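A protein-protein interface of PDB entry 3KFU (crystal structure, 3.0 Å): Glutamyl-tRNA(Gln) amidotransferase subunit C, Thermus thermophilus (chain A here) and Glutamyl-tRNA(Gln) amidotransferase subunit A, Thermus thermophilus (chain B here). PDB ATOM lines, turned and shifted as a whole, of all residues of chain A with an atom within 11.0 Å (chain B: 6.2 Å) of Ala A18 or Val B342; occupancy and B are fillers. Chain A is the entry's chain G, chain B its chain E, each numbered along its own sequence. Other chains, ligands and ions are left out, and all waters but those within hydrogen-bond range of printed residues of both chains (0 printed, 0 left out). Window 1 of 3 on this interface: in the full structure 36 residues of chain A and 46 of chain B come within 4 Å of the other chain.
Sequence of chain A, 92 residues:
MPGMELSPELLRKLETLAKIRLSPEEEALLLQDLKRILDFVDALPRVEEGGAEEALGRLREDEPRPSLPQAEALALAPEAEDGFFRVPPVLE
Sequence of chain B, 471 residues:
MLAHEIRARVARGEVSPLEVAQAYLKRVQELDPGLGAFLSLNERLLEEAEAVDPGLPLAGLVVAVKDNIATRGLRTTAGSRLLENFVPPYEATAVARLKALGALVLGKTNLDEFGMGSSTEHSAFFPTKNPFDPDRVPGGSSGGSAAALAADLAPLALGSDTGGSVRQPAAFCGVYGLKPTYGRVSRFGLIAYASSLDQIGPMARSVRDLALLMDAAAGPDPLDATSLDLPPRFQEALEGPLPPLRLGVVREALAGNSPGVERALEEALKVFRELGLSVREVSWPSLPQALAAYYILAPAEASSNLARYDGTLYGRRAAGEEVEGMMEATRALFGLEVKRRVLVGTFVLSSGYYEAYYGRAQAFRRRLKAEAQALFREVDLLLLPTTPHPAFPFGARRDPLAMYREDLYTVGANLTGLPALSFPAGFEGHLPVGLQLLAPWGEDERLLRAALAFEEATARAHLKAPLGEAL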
ATOM      1  N   GLU A   9       6.510  -1.573  12.445  1.00  0.00           N
ATOM      2  CA  GLU A   9       5.795  -0.434  11.884  1.00  0.00           C
ATOM      3  C   GLU A   9       6.431   0.016  10.575  1.00  0.00           C
ATOM      4  O   GLU A   9       5.734   0.313   9.606  1.00  0.00           O
ATOM      5  CB  GLU A   9       5.759   0.730  12.879  1.00  0.00           C
ATOM      6  CG  GLU A   9       4.772   0.550  14.024  1.00  0.00           C
ATOM      7  CD  GLU A   9       5.155  -0.578  14.960  1.00  0.00           C
ATOM      8  OE1 GLU A   9       6.355  -0.919  15.026  1.00  0.00           O
ATOM      9  OE2 GLU A   9       4.256  -1.126  15.632  1.00  0.00           O
ATOM     10  N   LEU A  10       7.759   0.067  10.552  1.00  0.00           N
ATOM     11  CA  LEU A  10       8.475   0.476   9.352  1.00  0.00           C
ATOM     12  C   LEU A  10       8.201  -0.493   8.211  1.00  0.00           C
ATOM     13  O   LEU A  10       7.920  -0.073   7.090  1.00  0.00           O
ATOM     14  CB  LEU A  10       9.977   0.582   9.616  1.00  0.00           C
ATOM     15  CG  LEU A  10      10.607   1.906   9.176  1.00  0.00           C
ATOM     16  CD1 LEU A  10      10.064   3.053  10.017  1.00  0.00           C
ATOM     17  CD2 LEU A  10      12.124   1.848   9.257  1.00  0.00           C
ATOM     18  N   LEU A  11       8.285  -1.788   8.497  1.00  0.00           N
ATOM     19  CA  LEU A  11       7.936  -2.803   7.511  1.00  0.00           C
ATOM     20  C   LEU A  11       6.579  -2.487   6.895  1.00  0.00           C
ATOM     21  O   LEU A  11       6.438  -2.441   5.673  1.00  0.00           O
ATOM     22  CB  LEU A  11       7.899  -4.190   8.149  1.00  0.00           C
ATOM     23  CG  LEU A  11       8.967  -5.168   7.671  1.00  0.00           C
ATOM     24  CD1 LEU A  11       8.657  -6.570   8.165  1.00  0.00           C
ATOM     25  CD2 LEU A  11       9.059  -5.142   6.156  1.00  0.00           C
ATOM     26  N   ARG A  12       5.583  -2.274   7.750  1.00  0.00           N
ATOM     27  CA  ARG A  12       4.254  -1.898   7.287  1.00  0.00           C
ATOM     28  C   ARG A  12       4.332  -0.666   6.393  1.00  0.00           C
ATOM     29  O   ARG A  12       3.733  -0.627   5.319  1.00  0.00           O
ATOM     30  CB  ARG A  12       3.318  -1.635   8.469  1.00  0.00           C
ATOM     31  CG  ARG A  12       2.746  -2.886   9.117  1.00  0.00           C
ATOM     32  CD  ARG A  12       1.670  -2.518  10.130  1.00  0.00           C
ATOM     33  NE  ARG A  12       0.910  -3.681  10.582  1.00  0.00           N
ATOM     34  CZ  ARG A  12      -0.200  -3.610  11.311  1.00  0.00           C
ATOM     35  NH1 ARG A  12      -0.687  -2.430  11.672  1.00  0.00           N
ATOM     36  NH2 ARG A  12      -0.827  -4.720  11.677  1.00  0.00           N
ATOM     37  N   LYS A  13       5.077   0.339   6.840  1.00  0.00           N
ATOM     38  CA  LYS A  13       5.245   1.561   6.069  1.00  0.00           C
ATOM     39  C   LYS A  13       5.904   1.260   4.727  1.00  0.00           C
ATOM     40  O   LYS A  13       5.475   1.759   3.685  1.00  0.00           O
ATOM     41  CB  LYS A  13       6.087   2.570   6.849  1.00  0.00           C
ATOM     42  CG  LYS A  13       6.197   3.931   6.182  1.00  0.00           C
ATOM     43  CD  LYS A  13       7.066   4.880   6.996  1.00  0.00           C
ATOM     44  CE  LYS A  13       7.061   6.287   6.410  1.00  0.00           C
ATOM     45  NZ  LYS A  13       5.720   6.933   6.498  1.00  0.00           N
ATOM     46  N   LEU A  14       6.947   0.439   4.759  1.00  0.00           N
ATOM     47  CA  LEU A  14       7.669   0.078   3.549  1.00  0.00           C
ATOM     48  C   LEU A  14       6.789  -0.712   2.591  1.00  0.00           C
ATOM     49  O   LEU A  14       6.682  -0.373   1.412  1.00  0.00           O
ATOM     50  CB  LEU A  14       8.930  -0.716   3.888  1.00  0.00           C
ATOM     51  CG  LEU A  14      10.002   0.052   4.663  1.00  0.00           C
ATOM     52  CD1 LEU A  14      11.187  -0.849   4.969  1.00  0.00           C
ATOM     53  CD2 LEU A  14      10.447   1.290   3.898  1.00  0.00           C
ATOM     54  N   GLU A  15       6.156  -1.764   3.096  1.00  0.00           N
ATOM     55  CA  GLU A  15       5.287  -2.576   2.252  1.00  0.00           C
ATOM     56  C   GLU A  15       4.152  -1.729   1.686  1.00  0.00           C
ATOM     57  O   GLU A  15       3.606  -2.032   0.627  1.00  0.00           O
ATOM     58  CB  GLU A  15       4.758  -3.797   3.009  1.00  0.00           C
ATOM     59  CG  GLU A  15       3.819  -3.482   4.150  1.00  0.00           C
ATOM     60  CD  GLU A  15       3.569  -4.689   5.032  1.00  0.00           C
ATOM     61  OE1 GLU A  15       2.389  -5.037   5.255  1.00  0.00           O
ATOM     62  OE2 GLU A  15       4.560  -5.291   5.503  1.00  0.00           O
ATOM     63  N   THR A  16       3.816  -0.654   2.390  1.00  0.00           N
ATOM     64  CA  THR A  16       2.833   0.299   1.896  1.00  0.00           C
ATOM     65  C   THR A  16       3.388   1.078   0.706  1.00  0.00           C
ATOM     66  O   THR A  16       2.781   1.102  -0.367  1.00  0.00           O
ATOM     67  CB  THR A  16       2.401   1.283   2.990  1.00  0.00           C
ATOM     68  OG1 THR A  16       1.666   0.579   3.996  1.00  0.00           O
ATOM     69  CG2 THR A  16       1.522   2.376   2.405  1.00  0.00           C
ATOM     70  N   LEU A  17       4.543   1.709   0.905  1.00  0.00           N
ATOM     71  CA  LEU A  17       5.202   2.478  -0.146  1.00  0.00           C
ATOM     72  C   LEU A  17       5.491   1.651  -1.396  1.00  0.00           C
ATOM     73  O   LEU A  17       5.435   2.167  -2.509  1.00  0.00           O
ATOM     74  CB  LEU A  17       6.500   3.088   0.380  1.00  0.00           C
ATOM     75  CG  LEU A  17       6.390   4.423   1.116  1.00  0.00           C
ATOM     76  CD1 LEU A  17       7.149   4.380   2.434  1.00  0.00           C
ATOM     77  CD2 LEU A  17       6.894   5.555   0.232  1.00  0.00           C
ATOM     78  N   ALA A  18       5.802   0.371  -1.208  1.00  0.00           N
ATOM     79  CA  ALA A  18       6.123  -0.511  -2.327  1.00  0.00           C
ATOM     80  C   ALA A  18       4.888  -1.202  -2.904  1.00  0.00           C
ATOM     81  O   ALA A  18       4.987  -1.955  -3.876  1.00  0.00           O
ATOM     82  CB  ALA A  18       7.151  -1.543  -1.902  1.00  0.00           C
ATOM     83  N   LYS A  19       3.731  -0.935  -2.301  1.00  0.00           N
ATOM     84  CA  LYS A  19       2.481  -1.607  -2.663  1.00  0.00           C
ATOM     85  C   LYS A  19       2.655  -3.115  -2.797  1.00  0.00           C
ATOM     86  O   LYS A  19       2.313  -3.706  -3.822  1.00  0.00           O
ATOM     87  CB  LYS A  19       1.868  -1.026  -3.941  1.00  0.00           C
ATOM     88  CG  LYS A  19       1.202   0.320  -3.743  1.00  0.00           C
ATOM     89  CD  LYS A  19       0.010   0.481  -4.665  1.00  0.00           C
ATOM     90  CE  LYS A  19      -0.679   1.816  -4.434  1.00  0.00           C
ATOM     91  NZ  LYS A  19      -1.002   2.032  -2.996  1.00  0.00           N
ATOM     92  N   ILE A  20       3.188  -3.729  -1.747  1.00  0.00           N
ATOM     93  CA  ILE A  20       3.388  -5.169  -1.718  1.00  0.00           C
ATOM     94  C   ILE A  20       2.708  -5.760  -0.493  1.00  0.00           C
ATOM     95  O   ILE A  20       3.074  -5.458   0.642  1.00  0.00           O
ATOM     96  CB  ILE A  20       4.883  -5.528  -1.722  1.00  0.00           C
ATOM     97  CG1 ILE A  20       5.523  -5.080  -3.039  1.00  0.00           C
ATOM     98  CG2 ILE A  20       5.072  -7.020  -1.514  1.00  0.00           C
ATOM     99  CD1 ILE A  20       6.978  -5.451  -3.175  1.00  0.00           C
ATOM    100  N   ARG A  21       1.703  -6.591  -0.734  1.00  0.00           N
ATOM    101  CA  ARG A  21       0.931  -7.192   0.343  1.00  0.00           C
ATOM    102  C   ARG A  21       1.473  -8.578   0.662  1.00  0.00           C
ATOM    103  O   ARG A  21       1.275  -9.519  -0.102  1.00  0.00           O
ATOM    104  CB  ARG A  21      -0.540  -7.285  -0.063  1.00  0.00           C
ATOM    105  CG  ARG A  21      -1.491  -7.662   1.058  1.00  0.00           C
ATOM    106  CD  ARG A  21      -2.883  -7.921   0.505  1.00  0.00           C
ATOM    107  NE  ARG A  21      -2.896  -9.081  -0.383  1.00  0.00           N
ATOM    108  CZ  ARG A  21      -3.892  -9.383  -1.209  1.00  0.00           C
ATOM    109  NH1 ARG A  21      -4.964  -8.604  -1.273  1.00  0.00           N
ATOM    110  NH2 ARG A  21      -3.812 -10.461  -1.976  1.00  0.00           N
ATOM    111  N   LEU A  22       2.169  -8.700   1.786  1.00  0.00           N
ATOM    112  CA  LEU A  22       2.693  -9.994   2.206  1.00  0.00           C
ATOM    113  C   LEU A  22       1.881 -10.587   3.348  1.00  0.00           C
ATOM    114  O   LEU A  22       1.261  -9.863   4.127  1.00  0.00           O
ATOM    115  CB  LEU A  22       4.171  -9.922   2.606  1.00  0.00           C
ATOM    116  CG  LEU A  22       4.880  -8.618   3.004  1.00  0.00           C
ATOM    117  CD1 LEU A  22       4.017  -7.494   3.565  1.00  0.00           C
ATOM    118  CD2 LEU A  22       6.178  -8.822   3.789  1.00  0.00           C
ATOM    119  N   LEU A  30      10.437 -11.956   6.712  1.00  0.00           N
ATOM    120  CA  LEU A  30      11.133 -10.824   6.117  1.00  0.00           C
ATOM    121  C   LEU A  30      11.642  -9.840   7.170  1.00  0.00           C
ATOM    122  O   LEU A  30      12.633  -9.146   6.955  1.00  0.00           O
ATOM    123  CB  LEU A  30      10.196 -10.114   5.143  1.00  0.00           C
ATOM    124  CG  LEU A  30      10.501 -10.261   3.648  1.00  0.00           C
ATOM    125  CD1 LEU A  30      11.342 -11.473   3.257  1.00  0.00           C
ATOM    126  CD2 LEU A  30       9.313 -10.011   2.715  1.00  0.00           C
ATOM    127  N   LEU A  34      15.422  -8.567   6.646  1.00  0.00           N
ATOM    128  CA  LEU A  34      15.674  -7.134   6.507  1.00  0.00           C
ATOM    129  C   LEU A  34      16.598  -6.589   7.594  1.00  0.00           C
ATOM    130  O   LEU A  34      17.474  -5.771   7.321  1.00  0.00           O
ATOM    131  CB  LEU A  34      14.356  -6.359   6.501  1.00  0.00           C
ATOM    132  CG  LEU A  34      13.656  -6.205   5.149  1.00  0.00           C
ATOM    133  CD1 LEU A  34      14.322  -5.116   4.328  1.00  0.00           C
ATOM    134  CD2 LEU A  34      13.629  -7.524   4.386  1.00  0.00           C
ATOM    135  N   ILE A  37      20.190  -7.763   6.870  1.00  0.00           N
ATOM    136  CA  ILE A  37      20.654  -7.086   5.665  1.00  0.00           C
ATOM    137  C   ILE A  37      20.967  -5.613   5.922  1.00  0.00           C
ATOM    138  O   ILE A  37      22.024  -5.122   5.533  1.00  0.00           O
ATOM    139  CB  ILE A  37      19.625  -7.207   4.529  1.00  0.00           C
ATOM    140  CG1 ILE A  37      19.447  -8.673   4.134  1.00  0.00           C
ATOM    141  CG2 ILE A  37      20.054  -6.384   3.331  1.00  0.00           C
ATOM    142  CD1 ILE A  37      18.461  -8.890   3.005  1.00  0.00           C
ATOM    143  N   LEU A  38      20.052  -4.912   6.583  1.00  0.00           N
ATOM    144  CA  LEU A  38      20.246  -3.495   6.871  1.00  0.00           C
ATOM    145  C   LEU A  38      21.415  -3.257   7.819  1.00  0.00           C
ATOM    146  O   LEU A  38      21.958  -2.156   7.882  1.00  0.00           O
ATOM    147  CB  LEU A  38      18.969  -2.872   7.436  1.00  0.00           C
ATOM    148  CG  LEU A  38      17.801  -2.791   6.453  1.00  0.00           C
ATOM    149  CD1 LEU A  38      16.635  -2.032   7.064  1.00  0.00           C
ATOM    150  CD2 LEU A  38      18.246  -2.133   5.163  1.00  0.00           C
ATOM    151  N   MET B 116      17.445 -11.368 -10.088  1.00  0.00           N
ATOM    152  CA  MET B 116      17.914 -11.300  -8.706  1.00  0.00           C
ATOM    153  C   MET B 116      18.005 -12.683  -8.067  1.00  0.00           C
ATOM    154  O   MET B 116      17.017 -13.232  -7.580  1.00  0.00           O
ATOM    155  CB  MET B 116      17.055 -10.344  -7.865  1.00  0.00           C
ATOM    156  CG  MET B 116      15.644 -10.139  -8.376  1.00  0.00           C
ATOM    157  SD  MET B 116      15.239  -8.391  -8.567  1.00  0.00           S
ATOM    158  CE  MET B 116      15.539  -7.796  -6.915  1.00  0.00           C
ATOM    159  N   PRO B 299      19.328  -2.525  -5.047  1.00  0.00           N
ATOM    160  CA  PRO B 299      17.942  -2.620  -4.582  1.00  0.00           C
ATOM    161  C   PRO B 299      17.189  -1.306  -4.775  1.00  0.00           C
ATOM    162  O   PRO B 299      16.018  -1.323  -5.153  1.00  0.00           O
ATOM    163  CB  PRO B 299      18.102  -2.934  -3.096  1.00  0.00           C
ATOM    164  CG  PRO B 299      19.412  -3.644  -3.014  1.00  0.00           C
ATOM    165  CD  PRO B 299      20.284  -2.942  -4.009  1.00  0.00           C
ATOM    166  N   ALA B 302      16.167  -1.095  -8.265  1.00  0.00           N
ATOM    167  CA  ALA B 302      15.260  -2.209  -8.510  1.00  0.00           C
ATOM    168  C   ALA B 302      13.833  -1.883  -8.094  1.00  0.00           C
ATOM    169  O   ALA B 302      12.885  -2.212  -8.803  1.00  0.00           O
ATOM    170  CB  ALA B 302      15.746  -3.459  -7.799  1.00  0.00           C
ATOM    171  N   SER B 303      13.676  -1.244  -6.941  1.00  0.00           N
ATOM    172  CA  SER B 303      12.347  -0.872  -6.471  1.00  0.00           C
ATOM    173  C   SER B 303      11.634   0.000  -7.503  1.00  0.00           C
ATOM    174  O   SER B 303      10.448  -0.184  -7.771  1.00  0.00           O
ATOM    175  CB  SER B 303      12.424  -0.145  -5.130  1.00  0.00           C
ATOM    176  OG  SER B 303      12.871   1.185  -5.300  1.00  0.00           O
ATOM    177  N   LEU B 306      10.952  -2.142 -10.860  1.00  0.00           N
ATOM    178  CA  LEU B 306       9.911  -3.152 -10.725  1.00  0.00           C
ATOM    179  C   LEU B 306       8.590  -2.551 -10.276  1.00  0.00           C
ATOM    180  O   LEU B 306       7.600  -3.263 -10.117  1.00  0.00           O
ATOM    181  CB  LEU B 306      10.349  -4.262  -9.771  1.00  0.00           C
ATOM    182  CG  LEU B 306      11.285  -5.290 -10.401  1.00  0.00           C
ATOM    183  CD1 LEU B 306      12.693  -4.733 -10.551  1.00  0.00           C
ATOM    184  CD2 LEU B 306      11.292  -6.550  -9.570  1.00  0.00           C
ATOM    185  N   ARG B 331       1.082  -7.503  -7.226  1.00  0.00           N
ATOM    186  CA  ARG B 331       2.483  -7.418  -6.840  1.00  0.00           C
ATOM    187  C   ARG B 331       2.828  -8.482  -5.803  1.00  0.00           C
ATOM    188  O   ARG B 331       3.988  -8.852  -5.644  1.00  0.00           O
ATOM    189  CB  ARG B 331       2.812  -6.015  -6.324  1.00  0.00           C
ATOM    190  CG  ARG B 331       2.665  -4.935  -7.379  1.00  0.00           C
ATOM    191  CD  ARG B 331       2.852  -3.544  -6.802  1.00  0.00           C
ATOM    192  NE  ARG B 331       4.219  -3.316  -6.346  1.00  0.00           N
ATOM    193  CZ  ARG B 331       5.258  -3.169  -7.163  1.00  0.00           C
ATOM    194  NH1 ARG B 331       5.087  -3.242  -8.476  1.00  0.00           N
ATOM    195  NH2 ARG B 331       6.470  -2.958  -6.667  1.00  0.00           N
ATOM    196  N   PHE B 334       5.013 -11.468  -6.682  1.00  0.00           N
ATOM    197  CA  PHE B 334       6.469 -11.457  -6.629  1.00  0.00           C
ATOM    198  C   PHE B 334       6.950 -12.616  -5.769  1.00  0.00           C
ATOM    199  O   PHE B 334       6.193 -13.151  -4.960  1.00  0.00           O
ATOM    200  CB  PHE B 334       6.984 -10.139  -6.044  1.00  0.00           C
ATOM    201  CG  PHE B 334       7.013  -9.007  -7.029  1.00  0.00           C
ATOM    202  CD1 PHE B 334       7.291  -9.240  -8.366  1.00  0.00           C
ATOM    203  CD2 PHE B 334       6.767  -7.709  -6.616  1.00  0.00           C
ATOM    204  CE1 PHE B 334       7.322  -8.200  -9.275  1.00  0.00           C
ATOM    205  CE2 PHE B 334       6.793  -6.664  -7.520  1.00  0.00           C
ATOM    206  CZ  PHE B 334       7.072  -6.910  -8.853  1.00  0.00           C
ATOM    207  N   GLU B 337      12.476 -13.410  -2.838  1.00  0.00           N
ATOM    208  CA  GLU B 337      13.704 -12.652  -3.039  1.00  0.00           C
ATOM    209  C   GLU B 337      13.406 -11.258  -3.572  1.00  0.00           C
ATOM    210  O   GLU B 337      13.934 -10.268  -3.063  1.00  0.00           O
ATOM    211  CB  GLU B 337      14.678 -13.387  -3.960  1.00  0.00           C
ATOM    212  CG  GLU B 337      16.009 -12.660  -4.151  1.00  0.00           C
ATOM    213  CD  GLU B 337      16.763 -12.439  -2.846  1.00  0.00           C
ATOM    214  OE1 GLU B 337      17.131 -13.435  -2.188  1.00  0.00           O
ATOM    215  OE2 GLU B 337      16.990 -11.266  -2.480  1.00  0.00           O
ATOM    216  N   VAL B 338      12.554 -11.175  -4.589  1.00  0.00           N
ATOM    217  CA  VAL B 338      12.206  -9.876  -5.154  1.00  0.00           C
ATOM    218  C   VAL B 338      11.675  -8.958  -4.063  1.00  0.00           C
ATOM    219  O   VAL B 338      12.218  -7.879  -3.837  1.00  0.00           O
ATOM    220  CB  VAL B 338      11.168  -9.982  -6.288  1.00  0.00           C
ATOM    221  CG1 VAL B 338      10.751  -8.596  -6.750  1.00  0.00           C
ATOM    222  CG2 VAL B 338      11.737 -10.784  -7.448  1.00  0.00           C
ATOM    223  N   LYS B 339      10.624  -9.404  -3.382  1.00  0.00           N
ATOM    224  CA  LYS B 339      10.024  -8.623  -2.306  1.00  0.00           C
ATOM    225  C   LYS B 339      11.108  -8.075  -1.393  1.00  0.00           C
ATOM    226  O   LYS B 339      11.166  -6.873  -1.115  1.00  0.00           O
ATOM    227  CB  LYS B 339       9.060  -9.483  -1.487  1.00  0.00           C
ATOM    228  CG  LYS B 339       7.902 -10.082  -2.273  1.00  0.00           C
ATOM    229  CD  LYS B 339       6.968 -10.848  -1.343  1.00  0.00           C
ATOM    230  CE  LYS B 339       6.075 -11.816  -2.106  1.00  0.00           C
ATOM    231  NZ  LYS B 339       5.217 -11.123  -3.099  1.00  0.00           N
ATOM    232  N   ARG B 340      11.970  -8.976  -0.939  1.00  0.00           N
ATOM    233  CA  ARG B 340      13.072  -8.628  -0.055  1.00  0.00           C
ATOM    234  C   ARG B 340      13.885  -7.447  -0.592  1.00  0.00           C
ATOM    235  O   ARG B 340      14.131  -6.477   0.125  1.00  0.00           O
ATOM    236  CB  ARG B 340      13.969  -9.852   0.161  1.00  0.00           C
ATOM    237  CG  ARG B 340      14.871  -9.754   1.372  1.00  0.00           C
ATOM    238  CD  ARG B 340      15.699 -11.015   1.567  1.00  0.00           C
ATOM    239  NE  ARG B 340      14.886 -12.166   1.955  1.00  0.00           N
ATOM    240  CZ  ARG B 340      14.686 -13.234   1.190  1.00  0.00           C
ATOM    241  NH1 ARG B 340      15.243 -13.304  -0.012  1.00  0.00           N
ATOM    242  NH2 ARG B 340      13.935 -14.236   1.630  1.00  0.00           N
ATOM    243  N   ARG B 341      14.285  -7.526  -1.857  1.00  0.00           N
ATOM    244  CA  ARG B 341      15.125  -6.490  -2.455  1.00  0.00           C
ATOM    245  C   ARG B 341      14.389  -5.160  -2.611  1.00  0.00           C
ATOM    246  O   ARG B 341      14.902  -4.117  -2.210  1.00  0.00           O
ATOM    247  CB  ARG B 341      15.685  -6.951  -3.804  1.00  0.00           C
ATOM    248  CG  ARG B 341      16.265  -8.360  -3.783  1.00  0.00           C
ATOM    249  CD  ARG B 341      17.757  -8.366  -3.507  1.00  0.00           C
ATOM    250  NE  ARG B 341      18.543  -8.414  -4.738  1.00  0.00           N
ATOM    251  CZ  ARG B 341      19.118  -9.512  -5.222  1.00  0.00           C
ATOM    252  NH1 ARG B 341      19.001 -10.666  -4.582  1.00  0.00           N
ATOM    253  NH2 ARG B 341      19.816  -9.455  -6.349  1.00  0.00           N
ATOM    254  N   VAL B 342      13.191  -5.190  -3.187  1.00  0.00           N
ATOM    255  CA  VAL B 342      12.429  -3.956  -3.391  1.00  0.00           C
ATOM    256  C   VAL B 342      11.975  -3.305  -2.076  1.00  0.00           C
ATOM    257  O   VAL B 342      11.764  -2.092  -2.019  1.00  0.00           O
ATOM    258  CB  VAL B 342      11.246  -4.140  -4.382  1.00  0.00           C
ATOM    259  CG1 VAL B 342      10.811  -5.584  -4.438  1.00  0.00           C
ATOM    260  CG2 VAL B 342      10.083  -3.236  -4.013  1.00  0.00           C
ATOM    261  N   LEU B 343      11.840  -4.096  -1.015  1.00  0.00           N
ATOM    262  CA  LEU B 343      11.605  -3.512   0.306  1.00  0.00           C
ATOM    263  C   LEU B 343      12.846  -2.769   0.794  1.00  0.00           C
ATOM    264  O   LEU B 343      12.747  -1.685   1.368  1.00  0.00           O
ATOM    265  CB  LEU B 343      11.166  -4.566   1.328  1.00  0.00           C
ATOM    266  CG  LEU B 343       9.721  -5.004   1.071  1.00  0.00           C
ATOM    267  CD1 LEU B 343       9.312  -6.359   1.646  1.00  0.00           C
ATOM    268  CD2 LEU B 343       8.674  -3.905   1.273  1.00  0.00           C
ATOM    269  N   VAL B 344      14.013  -3.359   0.561  1.00  0.00           N
ATOM    270  CA  VAL B 344      15.275  -2.701   0.873  1.00  0.00           C
ATOM    271  C   VAL B 344      15.429  -1.431   0.043  1.00  0.00           C
ATOM    272  O   VAL B 344      15.779  -0.372   0.566  1.00  0.00           O
ATOM    273  CB  VAL B 344      16.469  -3.631   0.597  1.00  0.00           C
ATOM    274  CG1 VAL B 344      17.766  -2.837   0.543  1.00  0.00           C
ATOM    275  CG2 VAL B 344      16.539  -4.731   1.645  1.00  0.00           C
ATOM    276  N   GLY B 345      15.158  -1.545  -1.251  1.00  0.00           N
ATOM    277  CA  GLY B 345      15.269  -0.421  -2.161  1.00  0.00           C
ATOM    278  C   GLY B 345      14.389   0.750  -1.773  1.00  0.00           C
ATOM    279  O   GLY B 345      14.792   1.907  -1.893  1.00  0.00           O
ATOM    280  N   THR B 346      13.181   0.456  -1.310  1.00  0.00           N
ATOM    281  CA  THR B 346      12.262   1.511  -0.904  1.00  0.00           C
ATOM    282  C   THR B 346      12.774   2.196   0.353  1.00  0.00           C
ATOM    283  O   THR B 346      12.660   3.412   0.494  1.00  0.00           O
ATOM    284  CB  THR B 346      10.835   0.980  -0.669  1.00  0.00           C
ATOM    285  OG1 THR B 346      10.894  -0.191   0.151  1.00  0.00           O
ATOM    286  CG2 THR B 346      10.171   0.628  -1.988  1.00  0.00           C
ATOM    287  N   PHE B 347      13.346   1.413   1.261  1.00  0.00           N
ATOM    288  CA  PHE B 347      13.888   1.954   2.505  1.00  0.00           C
ATOM    289  C   PHE B 347      15.067   2.892   2.264  1.00  0.00           C
ATOM    290  O   PHE B 347      15.128   3.988   2.818  1.00  0.00           O
ATOM    291  CB  PHE B 347      14.316   0.827   3.445  1.00  0.00           C
ATOM    292  CG  PHE B 347      15.082   1.302   4.646  1.00  0.00           C
ATOM    293  CD1 PHE B 347      14.421   1.682   5.801  1.00  0.00           C
ATOM    294  CD2 PHE B 347      16.467   1.373   4.619  1.00  0.00           C
ATOM    295  CE1 PHE B 347      15.125   2.124   6.905  1.00  0.00           C
ATOM    296  CE2 PHE B 347      17.179   1.814   5.723  1.00  0.00           C
ATOM    297  CZ  PHE B 347      16.506   2.190   6.865  1.00  0.00           C
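Ala B302 touches none of the printed residues of chain A. Ser B303 touches none of the printed residues of chain A. No residue of chain A comes within 4 Å of Leu B306. No residue of chain A comes within 4 Å of Val B338. Of the printed residues of chain A, Leu B343 touches Leu A14, Glu A15 and Leu A30. Of chain A, only Leu A34 comes within 4 Å of Val B344. Printed residues of chain B within 4 Å of Lys A19: Arg B331. Of the printed residues of chain B, Leu A30 touches Arg B340 (3.8 Å) and Leu B343 (3.8 Å). Pro B299 touches none of the printed residues of chain A. The nearest printed residue of chain B that does not touch Ala A18 is Leu B343 (4.2 Å). The nearest printed residue of chain A that does not touch Val B342 is Leu A14 (6.4 Å).
Among the printed residues, pairs that only touch across the chains: Leu A10 with Phe B347 (3.8 Å), Leu A14 with Leu B343 (3.9 Å), Leu A14 with Phe B347 (3.8 Å), Glu A15 with Leu B343 (3.8 Å), Ala A18 with Val B342 (3.99 Å), Ala A18 with Thr B346 (3.7 Å), Ile A20 with Arg B331 (3.97 Å), Ile A20 with Val B342 (3.9 Å), Leu A30 with Arg B340 (3.8 Å), Leu A30 with Leu B343 (3.8 Å), Leu A34 with Arg B340 (3.9 Å), Leu A34 with Val B344 (3.5 Å), Ile A37 with Arg B340 (3.8 Å) and Leu A38 with Phe B347 (3.97 Å).
The backbone carbonyl oxygen (O) of Ala A18 is in hydrogen-bond range of the guanidinium group (NE) of Arg B331, 2.9 Å away. O of Lys A19 lies close to NE of Arg B331.
The backbone carbonyl oxygen of Leu B306 lies within hydrogen-bond range of the guanidinium group of Arg B331. The side-chain carboxylate (OE1) of Glu B337 is in salt-bridge range of the guanidinium group (NH1) of Arg B340. The backbone carbonyl oxygen of Val B342 sits at hydrogen-bond distance from the side-chain hydroxyl of Thr B346. O of Leu B343 lies within hydrogen-bond range of OG1 of Thr B346, 2.7 Å away. The backbone carbonyl oxygen of Glu A15 lies within hydrogen-bond range of the backbone NH of Ile A20 (2.9 Å).
Printed residues of chain B that touch a printed residue of chain A: Arg B331, Arg B340, Val B342, Leu B343, Val B344, Thr B346 and Phe B347. Hydrophobic or aromatic side chains of chain A within 4 Å of the printed part of chain B: Leu A10, Leu A14, Ala A18, Ile A20, Leu A30, Leu A34, Ile A37 and Leu A38. Among the printed residues, 16 pairs touch across the chains.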
